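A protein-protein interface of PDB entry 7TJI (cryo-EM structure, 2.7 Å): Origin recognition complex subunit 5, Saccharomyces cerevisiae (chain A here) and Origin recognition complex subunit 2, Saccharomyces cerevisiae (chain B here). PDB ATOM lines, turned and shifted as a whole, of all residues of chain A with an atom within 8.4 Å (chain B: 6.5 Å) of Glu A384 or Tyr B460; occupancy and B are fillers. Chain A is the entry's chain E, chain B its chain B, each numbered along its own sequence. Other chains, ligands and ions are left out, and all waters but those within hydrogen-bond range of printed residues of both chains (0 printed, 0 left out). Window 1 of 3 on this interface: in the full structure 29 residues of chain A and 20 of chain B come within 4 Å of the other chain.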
ATOM      1  N   CYS A 338      -1.245  22.357 -20.771  1.00  0.00           N
ATOM      2  CA  CYS A 338      -2.502  21.728 -20.375  1.00  0.00           C
ATOM      3  C   CYS A 338      -3.642  22.735 -20.311  1.00  0.00           C
ATOM      4  O   CYS A 338      -4.783  22.412 -20.660  1.00  0.00           O
ATOM      5  CB  CYS A 338      -2.339  21.058 -19.014  1.00  0.00           C
ATOM      6  SG  CYS A 338      -1.482  19.504 -18.959  1.00  0.00           S
ATOM      7  N   ASP A 346      -4.004  15.914 -27.877  1.00  0.00           N
ATOM      8  CA  ASP A 346      -2.749  15.577 -27.203  1.00  0.00           C
ATOM      9  C   ASP A 346      -1.984  14.480 -27.935  1.00  0.00           C
ATOM     10  O   ASP A 346      -0.759  14.563 -28.075  1.00  0.00           O
ATOM     11  CB  ASP A 346      -3.025  15.150 -25.763  1.00  0.00           C
ATOM     12  CG  ASP A 346      -2.940  16.305 -24.780  1.00  0.00           C
ATOM     13  OD1 ASP A 346      -2.495  17.398 -25.179  1.00  0.00           O
ATOM     14  OD2 ASP A 346      -3.314  16.112 -23.604  1.00  0.00           O
ATOM     15  N   PHE A 381      -7.456  21.358 -15.704  1.00  0.00           N
ATOM     16  CA  PHE A 381      -6.951  20.045 -16.086  1.00  0.00           C
ATOM     17  C   PHE A 381      -6.752  19.179 -14.848  1.00  0.00           C
ATOM     18  O   PHE A 381      -6.710  19.670 -13.718  1.00  0.00           O
ATOM     19  CB  PHE A 381      -5.638  20.148 -16.890  1.00  0.00           C
ATOM     20  CG  PHE A 381      -4.557  20.967 -16.216  1.00  0.00           C
ATOM     21  CD1 PHE A 381      -3.664  20.377 -15.327  1.00  0.00           C
ATOM     22  CD2 PHE A 381      -4.424  22.320 -16.488  1.00  0.00           C
ATOM     23  CE1 PHE A 381      -2.681  21.124 -14.714  1.00  0.00           C
ATOM     24  CE2 PHE A 381      -3.437  23.065 -15.883  1.00  0.00           C
ATOM     25  CZ  PHE A 381      -2.569  22.470 -14.993  1.00  0.00           C
ATOM     26  N   ALA A 382      -6.622  17.876 -15.086  1.00  0.00           N
ATOM     27  CA  ALA A 382      -6.349  16.887 -14.054  1.00  0.00           C
ATOM     28  C   ALA A 382      -4.847  16.739 -13.817  1.00  0.00           C
ATOM     29  O   ALA A 382      -4.016  17.244 -14.572  1.00  0.00           O
ATOM     30  CB  ALA A 382      -6.962  15.540 -14.434  1.00  0.00           C
ATOM     31  N   ILE A 383      -4.509  16.024 -12.739  1.00  0.00           N
ATOM     32  CA  ILE A 383      -3.111  15.813 -12.364  1.00  0.00           C
ATOM     33  C   ILE A 383      -2.416  14.889 -13.359  1.00  0.00           C
ATOM     34  O   ILE A 383      -1.267  15.132 -13.758  1.00  0.00           O
ATOM     35  CB  ILE A 383      -3.036  15.275 -10.917  1.00  0.00           C
ATOM     36  CG1 ILE A 383      -3.115  16.423  -9.917  1.00  0.00           C
ATOM     37  CG2 ILE A 383      -1.761  14.493 -10.646  1.00  0.00           C
ATOM     38  CD1 ILE A 383      -2.059  17.490 -10.111  1.00  0.00           C
ATOM     39  N   GLU A 384      -3.112  13.841 -13.805  1.00  0.00           N
ATOM     40  CA  GLU A 384      -2.474  12.794 -14.597  1.00  0.00           C
ATOM     41  C   GLU A 384      -2.149  13.269 -16.009  1.00  0.00           C
ATOM     42  O   GLU A 384      -1.117  12.884 -16.570  1.00  0.00           O
ATOM     43  CB  GLU A 384      -3.368  11.553 -14.630  1.00  0.00           C
ATOM     44  CG  GLU A 384      -2.715  10.310 -15.224  1.00  0.00           C
ATOM     45  CD  GLU A 384      -1.960   9.478 -14.199  1.00  0.00           C
ATOM     46  OE1 GLU A 384      -1.661   9.986 -13.099  1.00  0.00           O
ATOM     47  OE2 GLU A 384      -1.667   8.301 -14.495  1.00  0.00           O
ATOM     48  N   ARG A 385      -3.010  14.108 -16.594  1.00  0.00           N
ATOM     49  CA  ARG A 385      -2.696  14.731 -17.879  1.00  0.00           C
ATOM     50  C   ARG A 385      -1.485  15.647 -17.767  1.00  0.00           C
ATOM     51  O   ARG A 385      -0.642  15.690 -18.676  1.00  0.00           O
ATOM     52  CB  ARG A 385      -3.899  15.514 -18.393  1.00  0.00           C
ATOM     53  CG  ARG A 385      -3.690  16.115 -19.763  1.00  0.00           C
ATOM     54  CD  ARG A 385      -4.652  17.236 -20.017  1.00  0.00           C
ATOM     55  NE  ARG A 385      -4.372  17.901 -21.280  1.00  0.00           N
ATOM     56  CZ  ARG A 385      -4.943  19.031 -21.669  1.00  0.00           C
ATOM     57  NH1 ARG A 385      -5.854  19.634 -20.923  1.00  0.00           N
ATOM     58  NH2 ARG A 385      -4.586  19.572 -22.828  1.00  0.00           N
ATOM     59  N   LEU A 386      -1.385  16.383 -16.655  1.00  0.00           N
ATOM     60  CA  LEU A 386      -0.222  17.229 -16.411  1.00  0.00           C
ATOM     61  C   LEU A 386       1.048  16.396 -16.296  1.00  0.00           C
ATOM     62  O   LEU A 386       2.087  16.770 -16.845  1.00  0.00           O
ATOM     63  CB  LEU A 386      -0.445  18.077 -15.157  1.00  0.00           C
ATOM     64  CG  LEU A 386       0.772  18.759 -14.531  1.00  0.00           C
ATOM     65  CD1 LEU A 386       1.332  19.817 -15.458  1.00  0.00           C
ATOM     66  CD2 LEU A 386       0.416  19.365 -13.191  1.00  0.00           C
ATOM     67  N   LEU A 387       0.969  15.243 -15.630  1.00  0.00           N
ATOM     68  CA  LEU A 387       2.124  14.354 -15.529  1.00  0.00           C
ATOM     69  C   LEU A 387       2.501  13.749 -16.882  1.00  0.00           C
ATOM     70  O   LEU A 387       3.690  13.624 -17.198  1.00  0.00           O
ATOM     71  CB  LEU A 387       1.840  13.259 -14.504  1.00  0.00           C
ATOM     72  CG  LEU A 387       1.720  13.742 -13.057  1.00  0.00           C
ATOM     73  CD1 LEU A 387       1.388  12.588 -12.126  1.00  0.00           C
ATOM     74  CD2 LEU A 387       2.991  14.445 -12.627  1.00  0.00           C
ATOM     75  N   ALA A 388       1.502  13.377 -17.687  1.00  0.00           N
ATOM     76  CA  ALA A 388       1.756  12.806 -19.010  1.00  0.00           C
ATOM     77  C   ALA A 388       2.411  13.819 -19.946  1.00  0.00           C
ATOM     78  O   ALA A 388       3.347  13.481 -20.682  1.00  0.00           O
ATOM     79  CB  ALA A 388       0.450  12.293 -19.609  1.00  0.00           C
ATOM     80  N   ILE A 389       1.948  15.069 -19.917  1.00  0.00           N
ATOM     81  CA  ILE A 389       2.555  16.102 -20.745  1.00  0.00           C
ATOM     82  C   ILE A 389       3.924  16.510 -20.194  1.00  0.00           C
ATOM     83  O   ILE A 389       4.849  16.803 -20.963  1.00  0.00           O
ATOM     84  CB  ILE A 389       1.566  17.277 -20.906  1.00  0.00           C
ATOM     85  CG1 ILE A 389       0.451  16.845 -21.861  1.00  0.00           C
ATOM     86  CG2 ILE A 389       2.219  18.562 -21.401  1.00  0.00           C
ATOM     87  CD1 ILE A 389      -0.664  17.822 -22.020  1.00  0.00           C
ATOM     88  N   PHE A 390       4.095  16.473 -18.865  1.00  0.00           N
ATOM     89  CA  PHE A 390       5.387  16.775 -18.251  1.00  0.00           C
ATOM     90  C   PHE A 390       6.453  15.761 -18.649  1.00  0.00           C
ATOM     91  O   PHE A 390       7.581  16.133 -18.987  1.00  0.00           O
ATOM     92  CB  PHE A 390       5.238  16.827 -16.725  1.00  0.00           C
ATOM     93  CG  PHE A 390       6.549  16.793 -15.971  1.00  0.00           C
ATOM     94  CD1 PHE A 390       7.303  17.944 -15.826  1.00  0.00           C
ATOM     95  CD2 PHE A 390       7.006  15.619 -15.377  1.00  0.00           C
ATOM     96  CE1 PHE A 390       8.499  17.923 -15.127  1.00  0.00           C
ATOM     97  CE2 PHE A 390       8.201  15.593 -14.687  1.00  0.00           C
ATOM     98  CZ  PHE A 390       8.946  16.745 -14.558  1.00  0.00           C
ATOM     99  N   GLN A 391       6.123  14.474 -18.605  1.00  0.00           N
ATOM    100  CA  GLN A 391       7.108  13.485 -19.019  1.00  0.00           C
ATOM    101  C   GLN A 391       7.168  13.319 -20.530  1.00  0.00           C
ATOM    102  O   GLN A 391       8.119  12.709 -21.028  1.00  0.00           O
ATOM    103  CB  GLN A 391       6.846  12.139 -18.334  1.00  0.00           C
ATOM    104  CG  GLN A 391       5.752  11.302 -18.950  1.00  0.00           C
ATOM    105  CD  GLN A 391       6.000   9.809 -18.793  1.00  0.00           C
ATOM    106  OE1 GLN A 391       7.135   9.372 -18.624  1.00  0.00           O
ATOM    107  NE2 GLN A 391       4.933   9.021 -18.844  1.00  0.00           N
ATOM    108  N   ALA A 416       7.071  10.023 -12.161  1.00  0.00           N
ATOM    109  CA  ALA A 416       6.687  11.044 -11.188  1.00  0.00           C
ATOM    110  C   ALA A 416       6.972  10.504  -9.791  1.00  0.00           C
ATOM    111  O   ALA A 416       6.153   9.814  -9.187  1.00  0.00           O
ATOM    112  CB  ALA A 416       5.222  11.427 -11.353  1.00  0.00           C
ATOM    113  N   PHE A 421       6.183  15.535  -7.211  1.00  0.00           N
ATOM    114  CA  PHE A 421       5.013  15.940  -6.441  1.00  0.00           C
ATOM    115  C   PHE A 421       5.352  17.029  -5.435  1.00  0.00           C
ATOM    116  O   PHE A 421       4.522  17.911  -5.181  1.00  0.00           O
ATOM    117  CB  PHE A 421       4.403  14.724  -5.753  1.00  0.00           C
ATOM    118  CG  PHE A 421       3.554  13.895  -6.663  1.00  0.00           C
ATOM    119  CD1 PHE A 421       4.115  12.877  -7.417  1.00  0.00           C
ATOM    120  CD2 PHE A 421       2.199  14.150  -6.789  1.00  0.00           C
ATOM    121  CE1 PHE A 421       3.334  12.116  -8.266  1.00  0.00           C
ATOM    122  CE2 PHE A 421       1.415  13.395  -7.637  1.00  0.00           C
ATOM    123  CZ  PHE A 421       1.983  12.376  -8.376  1.00  0.00           C
ATOM    124  N   LEU A 424       5.436  20.190  -7.525  1.00  0.00           N
ATOM    125  CA  LEU A 424       4.077  20.611  -7.856  1.00  0.00           C
ATOM    126  C   LEU A 424       3.376  21.237  -6.653  1.00  0.00           C
ATOM    127  O   LEU A 424       2.661  22.243  -6.792  1.00  0.00           O
ATOM    128  CB  LEU A 424       3.297  19.411  -8.387  1.00  0.00           C
ATOM    129  CG  LEU A 424       1.904  19.558  -8.999  1.00  0.00           C
ATOM    130  CD1 LEU A 424       1.782  20.782  -9.889  1.00  0.00           C
ATOM    131  CD2 LEU A 424       1.586  18.298  -9.772  1.00  0.00           C
ATOM    132  N   SER A 425       3.586  20.663  -5.462  1.00  0.00           N
ATOM    133  CA  SER A 425       3.055  21.241  -4.231  1.00  0.00           C
ATOM    134  C   SER A 425       3.660  22.613  -3.957  1.00  0.00           C
ATOM    135  O   SER A 425       2.961  23.530  -3.501  1.00  0.00           O
ATOM    136  CB  SER A 425       3.321  20.293  -3.063  1.00  0.00           C
ATOM    137  OG  SER A 425       2.323  20.399  -2.066  1.00  0.00           O
ATOM    138  N   TYR A 443      -5.928  18.368  -1.666  1.00  0.00           N
ATOM    139  CA  TYR A 443      -5.189  18.079  -2.887  1.00  0.00           C
ATOM    140  C   TYR A 443      -5.549  16.733  -3.491  1.00  0.00           C
ATOM    141  O   TYR A 443      -5.345  16.530  -4.691  1.00  0.00           O
ATOM    142  CB  TYR A 443      -3.690  18.109  -2.597  1.00  0.00           C
ATOM    143  CG  TYR A 443      -3.164  19.472  -2.241  1.00  0.00           C
ATOM    144  CD1 TYR A 443      -3.245  20.523  -3.146  1.00  0.00           C
ATOM    145  CD2 TYR A 443      -2.595  19.717  -0.995  1.00  0.00           C
ATOM    146  CE1 TYR A 443      -2.766  21.776  -2.825  1.00  0.00           C
ATOM    147  CE2 TYR A 443      -2.112  20.969  -0.665  1.00  0.00           C
ATOM    148  CZ  TYR A 443      -2.206  21.994  -1.584  1.00  0.00           C
ATOM    149  OH  TYR A 443      -1.730  23.242  -1.268  1.00  0.00           O
ATOM    150  N   LEU A 444      -6.080  15.815  -2.693  1.00  0.00           N
ATOM    151  CA  LEU A 444      -6.121  14.407  -3.056  1.00  0.00           C
ATOM    152  C   LEU A 444      -7.428  13.990  -3.707  1.00  0.00           C
ATOM    153  O   LEU A 444      -7.539  12.845  -4.157  1.00  0.00           O
ATOM    154  CB  LEU A 444      -5.865  13.562  -1.803  1.00  0.00           C
ATOM    155  CG  LEU A 444      -4.478  13.594  -1.140  1.00  0.00           C
ATOM    156  CD1 LEU A 444      -4.151  12.250  -0.548  1.00  0.00           C
ATOM    157  CD2 LEU A 444      -3.368  13.993  -2.100  1.00  0.00           C
ATOM    158  N   SER A 445      -8.410  14.883  -3.772  1.00  0.00           N
ATOM    159  CA  SER A 445      -9.702  14.532  -4.339  1.00  0.00           C
ATOM    160  C   SER A 445      -9.613  14.461  -5.862  1.00  0.00           C
ATOM    161  O   SER A 445      -8.894  15.252  -6.482  1.00  0.00           O
ATOM    162  CB  SER A 445     -10.756  15.556  -3.927  1.00  0.00           C
ATOM    163  OG  SER A 445     -11.999  15.289  -4.548  1.00  0.00           O
ATOM    164  N   PRO A 446     -10.329  13.529  -6.497  1.00  0.00           N
ATOM    165  CA  PRO A 446     -10.366  13.489  -7.963  1.00  0.00           C
ATOM    166  C   PRO A 446     -11.296  14.519  -8.583  1.00  0.00           C
ATOM    167  O   PRO A 446     -11.349  14.618  -9.813  1.00  0.00           O
ATOM    168  CB  PRO A 446     -10.856  12.057  -8.260  1.00  0.00           C
ATOM    169  CG  PRO A 446     -10.900  11.348  -6.933  1.00  0.00           C
ATOM    170  CD  PRO A 446     -11.080  12.411  -5.912  1.00  0.00           C
ATOM    171  N   VAL A 448     -10.905  17.745  -7.864  1.00  0.00           N
ATOM    172  CA  VAL A 448     -10.147  18.986  -7.757  1.00  0.00           C
ATOM    173  C   VAL A 448      -9.390  19.192  -9.059  1.00  0.00           C
ATOM    174  O   VAL A 448      -8.612  18.327  -9.479  1.00  0.00           O
ATOM    175  CB  VAL A 448      -9.190  18.953  -6.556  1.00  0.00           C
ATOM    176  CG1 VAL A 448      -8.203  20.104  -6.622  1.00  0.00           C
ATOM    177  CG2 VAL A 448      -9.975  19.001  -5.268  1.00  0.00           C
ATOM    178  N   TRP A 450      -7.088  21.860 -11.799  1.00  0.00           N
ATOM    179  CA  TRP A 450      -5.815  22.559 -11.743  1.00  0.00           C
ATOM    180  C   TRP A 450      -5.701  23.497 -12.931  1.00  0.00           C
ATOM    181  O   TRP A 450      -6.165  23.174 -14.025  1.00  0.00           O
ATOM    182  CB  TRP A 450      -4.706  21.514 -11.736  1.00  0.00           C
ATOM    183  CG  TRP A 450      -4.693  20.734 -10.466  1.00  0.00           C
ATOM    184  CD1 TRP A 450      -5.107  19.453 -10.294  1.00  0.00           C
ATOM    185  CD2 TRP A 450      -4.048  21.110  -9.245  1.00  0.00           C
ATOM    186  NE1 TRP A 450      -4.895  19.058  -9.000  1.00  0.00           N
ATOM    187  CE2 TRP A 450      -4.214  20.045  -8.343  1.00  0.00           C
ATOM    188  CE3 TRP A 450      -3.376  22.256  -8.819  1.00  0.00           C
ATOM    189  CZ2 TRP A 450      -3.739  20.092  -7.036  1.00  0.00           C
ATOM    190  CZ3 TRP A 450      -2.901  22.303  -7.523  1.00  0.00           C
ATOM    191  CH2 TRP A 450      -3.091  21.229  -6.643  1.00  0.00           C
ATOM    192  N   TYR B 246      -1.621   6.755 -21.964  1.00  0.00           N
ATOM    193  CA  TYR B 246      -2.608   7.702 -21.461  1.00  0.00           C
ATOM    194  C   TYR B 246      -3.352   8.382 -22.601  1.00  0.00           C
ATOM    195  O   TYR B 246      -4.585   8.448 -22.593  1.00  0.00           O
ATOM    196  CB  TYR B 246      -1.941   8.753 -20.579  1.00  0.00           C
ATOM    197  CG  TYR B 246      -2.905   9.819 -20.109  1.00  0.00           C
ATOM    198  CD1 TYR B 246      -3.873   9.527 -19.164  1.00  0.00           C
ATOM    199  CD2 TYR B 246      -2.853  11.114 -20.618  1.00  0.00           C
ATOM    200  CE1 TYR B 246      -4.759  10.490 -18.723  1.00  0.00           C
ATOM    201  CE2 TYR B 246      -3.742  12.089 -20.188  1.00  0.00           C
ATOM    202  CZ  TYR B 246      -4.687  11.768 -19.238  1.00  0.00           C
ATOM    203  OH  TYR B 246      -5.578  12.716 -18.801  1.00  0.00           O
ATOM    204  N   ARG B 250      -7.615   7.262 -24.110  1.00  0.00           N
ATOM    205  CA  ARG B 250      -8.683   8.263 -24.145  1.00  0.00           C
ATOM    206  C   ARG B 250      -9.101   8.560 -25.584  1.00  0.00           C
ATOM    207  O   ARG B 250      -9.049   9.693 -26.057  1.00  0.00           O
ATOM    208  CB  ARG B 250      -8.246   9.535 -23.431  1.00  0.00           C
ATOM    209  CG  ARG B 250      -7.699   9.313 -22.046  1.00  0.00           C
ATOM    210  CD  ARG B 250      -6.954  10.540 -21.582  1.00  0.00           C
ATOM    211  NE  ARG B 250      -7.861  11.610 -21.192  1.00  0.00           N
ATOM    212  CZ  ARG B 250      -8.365  11.755 -19.975  1.00  0.00           C
ATOM    213  NH1 ARG B 250      -8.054  10.923 -18.996  1.00  0.00           N
ATOM    214  NH2 ARG B 250      -9.204  12.759 -19.734  1.00  0.00           N
ATOM    215  N   ASP B 457      -2.012   5.877   2.221  1.00  0.00           N
ATOM    216  CA  ASP B 457      -2.678   4.916   1.353  1.00  0.00           C
ATOM    217  C   ASP B 457      -2.962   5.432  -0.048  1.00  0.00           C
ATOM    218  O   ASP B 457      -2.984   4.633  -0.986  1.00  0.00           O
ATOM    219  CB  ASP B 457      -4.001   4.457   1.982  1.00  0.00           C
ATOM    220  CG  ASP B 457      -3.876   3.128   2.689  1.00  0.00           C
ATOM    221  OD1 ASP B 457      -2.881   2.419   2.439  1.00  0.00           O
ATOM    222  OD2 ASP B 457      -4.772   2.791   3.488  1.00  0.00           O
ATOM    223  N   HIS B 458      -3.177   6.733  -0.218  1.00  0.00           N
ATOM    224  CA  HIS B 458      -3.502   7.279  -1.529  1.00  0.00           C
ATOM    225  C   HIS B 458      -2.265   7.323  -2.415  1.00  0.00           C
ATOM    226  O   HIS B 458      -1.161   7.612  -1.950  1.00  0.00           O
ATOM    227  CB  HIS B 458      -4.093   8.678  -1.384  1.00  0.00           C
ATOM    228  CG  HIS B 458      -4.979   9.084  -2.519  1.00  0.00           C
ATOM    229  ND1 HIS B 458      -4.488   9.601  -3.697  1.00  0.00           N
ATOM    230  CD2 HIS B 458      -6.324   9.062  -2.650  1.00  0.00           C
ATOM    231  CE1 HIS B 458      -5.494   9.871  -4.509  1.00  0.00           C
ATOM    232  NE2 HIS B 458      -6.619   9.555  -3.895  1.00  0.00           N
ATOM    233  N   ILE B 459      -2.460   7.042  -3.706  1.00  0.00           N
ATOM    234  CA  ILE B 459      -1.344   7.009  -4.646  1.00  0.00           C
ATOM    235  C   ILE B 459      -0.814   8.409  -4.957  1.00  0.00           C
ATOM    236  O   ILE B 459       0.306   8.545  -5.460  1.00  0.00           O
ATOM    237  CB  ILE B 459      -1.764   6.255  -5.929  1.00  0.00           C
ATOM    238  CG1 ILE B 459      -0.548   5.611  -6.597  1.00  0.00           C
ATOM    239  CG2 ILE B 459      -2.505   7.164  -6.902  1.00  0.00           C
ATOM    240  CD1 ILE B 459      -0.877   4.656  -7.686  1.00  0.00           C
ATOM    241  N   TYR B 460      -1.582   9.453  -4.654  1.00  0.00           N
ATOM    242  CA  TYR B 460      -1.185  10.834  -4.884  1.00  0.00           C
ATOM    243  C   TYR B 460      -0.758  11.543  -3.607  1.00  0.00           C
ATOM    244  O   TYR B 460      -0.666  12.772  -3.607  1.00  0.00           O
ATOM    245  CB  TYR B 460      -2.334  11.610  -5.526  1.00  0.00           C
ATOM    246  CG  TYR B 460      -2.468  11.454  -7.019  1.00  0.00           C
ATOM    247  CD1 TYR B 460      -1.559  10.702  -7.752  1.00  0.00           C
ATOM    248  CD2 TYR B 460      -3.538  12.032  -7.689  1.00  0.00           C
ATOM    249  CE1 TYR B 460      -1.699  10.555  -9.115  1.00  0.00           C
ATOM    250  CE2 TYR B 460      -3.690  11.884  -9.047  1.00  0.00           C
ATOM    251  CZ  TYR B 460      -2.768  11.148  -9.757  1.00  0.00           C
ATOM    252  OH  TYR B 460      -2.932  11.013 -11.115  1.00  0.00           O
ATOM    253  N   ALA B 461      -0.533  10.797  -2.524  1.00  0.00           N
ATOM    254  CA  ALA B 461      -0.167  11.365  -1.224  1.00  0.00           C
ATOM    255  C   ALA B 461       1.045  12.311  -1.191  1.00  0.00           C
ATOM    256  O   ALA B 461       0.964  13.316  -0.460  1.00  0.00           O
ATOM    257  CB  ALA B 461       0.026  10.223  -0.212  1.00  0.00           C
ATOM    258  N   PRO B 462       2.158  12.096  -1.923  1.00  0.00           N
ATOM    259  CA  PRO B 462       3.259  13.082  -1.879  1.00  0.00           C
ATOM    260  C   PRO B 462       2.925  14.472  -2.415  1.00  0.00           C
ATOM    261  O   PRO B 462       3.727  15.391  -2.210  1.00  0.00           O
ATOM    262  CB  PRO B 462       4.347  12.428  -2.731  1.00  0.00           C
ATOM    263  CG  PRO B 462       4.074  11.018  -2.630  1.00  0.00           C
ATOM    264  CD  PRO B 462       2.625  10.884  -2.633  1.00  0.00           C
ATOM    265  N   LEU B 463       1.775  14.658  -3.071  1.00  0.00           N
ATOM    266  CA  LEU B 463       1.304  15.988  -3.436  1.00  0.00           C
ATOM    267  C   LEU B 463       0.962  16.849  -2.223  1.00  0.00           C
ATOM    268  O   LEU B 463       0.884  18.075  -2.356  1.00  0.00           O
ATOM    269  CB  LEU B 463       0.082  15.862  -4.347  1.00  0.00           C
ATOM    270  CG  LEU B 463      -0.378  17.036  -5.204  1.00  0.00           C
ATOM    271  CD1 LEU B 463       0.714  17.432  -6.164  1.00  0.00           C
ATOM    272  CD2 LEU B 463      -1.645  16.669  -5.942  1.00  0.00           C
ATOM    273  N   LEU B 464       0.765  16.246  -1.043  1.00  0.00           N
ATOM    274  CA  LEU B 464       0.419  17.029   0.139  1.00  0.00           C
ATOM    275  C   LEU B 464       1.568  17.894   0.648  1.00  0.00           C
ATOM    276  O   LEU B 464       1.316  18.883   1.343  1.00  0.00           O
ATOM    277  CB  LEU B 464      -0.053  16.104   1.261  1.00  0.00           C
ATOM    278  CG  LEU B 464      -1.406  15.414   1.080  1.00  0.00           C
ATOM    279  CD1 LEU B 464      -1.672  14.461   2.227  1.00  0.00           C
ATOM    280  CD2 LEU B 464      -2.517  16.445   0.957  1.00  0.00           C
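Phe A381 touches none of the printed residues of chain B.
Glu A384 touches just one residue of chain B: Tyr B460 (2.6 Å).
Printed residues of chain B within 4 Å of Arg A385: Tyr B246 (3.3 Å).
Of the printed residues of chain B, Leu A424 touches Leu B463 (3.7 Å).
Of the printed residues of chain B, Tyr A443 touches Leu B463 and Leu B464.
Printed residues of chain A within 4 Å of Tyr B246: Arg A385 (3.3 Å) and Ala A388 (3.6 Å).
Asp B457 touches none of the printed residues of chain A.
Of the printed residues of chain A, His B458 touches Leu A444 (3.4 Å).
Tyr B460 touches just these residues of chain A: Ile A383 (3.6 Å), Glu A384 (2.6 Å), Phe A421 (3.97 Å) and Leu A444 (3.3 Å).
No residue of chain A comes within 4 Å of Ala B461.
The nearest residue of chain B that does not touch Glu A384 is Tyr B246 (4.1 Å).
A ring nitrogen (NE2) of His B458 is in hydrogen-bond range of the backbone carbonyl oxygen (O) of Leu A444, at 3.4 Å.
The side-chain hydroxyl of Tyr B460 lies within hydrogen-bond range of the side-chain carboxylate of Glu A384, 2.6 Å away.
The backbone carbonyl oxygen (O) of Leu B463 is in hydrogen-bond range of the side-chain hydroxyl (OG) of Ser A425, 2.7 Å away.
Hydrophobic or aromatic side chains of chain B that line the printed part of chain A: Tyr B246, His B458, Tyr B460, Pro B462, Leu B463 and Leu B464.
Printed residues of chain A that touch a printed residue of chain B: Ile A383, Glu A384, Arg A385, Ala A388, Phe A421, Leu A424, Ser A425, Tyr A443 and Leu A444.
Hydrophobic or aromatic side chains of chain A within 4 Å of the printed part of chain B: Ile A383, Ala A388, Phe A421, Leu A424, Tyr A443 and Leu A444.
Among the printed residues, no Asp or Glu carboxylate lies within 4 Å of a Lys or Arg side-chain nitrogen of the other chain.
The side-chain hydroxyl (OH) of Tyr B246 is in hydrogen-bond range of the guanidinium group (NH1) of Arg B250 (3.1 Å).
A ring nitrogen (ND1) of His B458 lies within hydrogen-bond range of the backbone NH of Tyr B460, 3.1 Å away.
The backbone carbonyl oxygen (O) of Cys A338 sits at hydrogen-bond distance from the guanidinium group (NH1) of Arg A385, at 3.0 Å.
OD2 of Asp A346 is in salt-bridge range of NE of Arg A385 (3.1 Å).
Ile A383 touches Tyr B460.
Ala A388 touches Tyr B246 (CB to CD2, 3.6 Å).
Phe A421 touches Tyr B460.
C of Pro B462 touches CB of Phe A421 (3.7 Å).
CG of Leu A424 touches CD1 of Leu B463, 3.7 Å away.
OG of Ser A425 touches C of Leu B464, 3.8 Å away.
Leu B463 touches Tyr A443 (CD2 to O, 3.9 Å).
Leu B464 touches Tyr A443.
Leu A444 touches Tyr B460 (CD2 to O, 3.3 Å).
Leu A444 touches Leu B464 (CD2 to CG, 3.998 Å).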
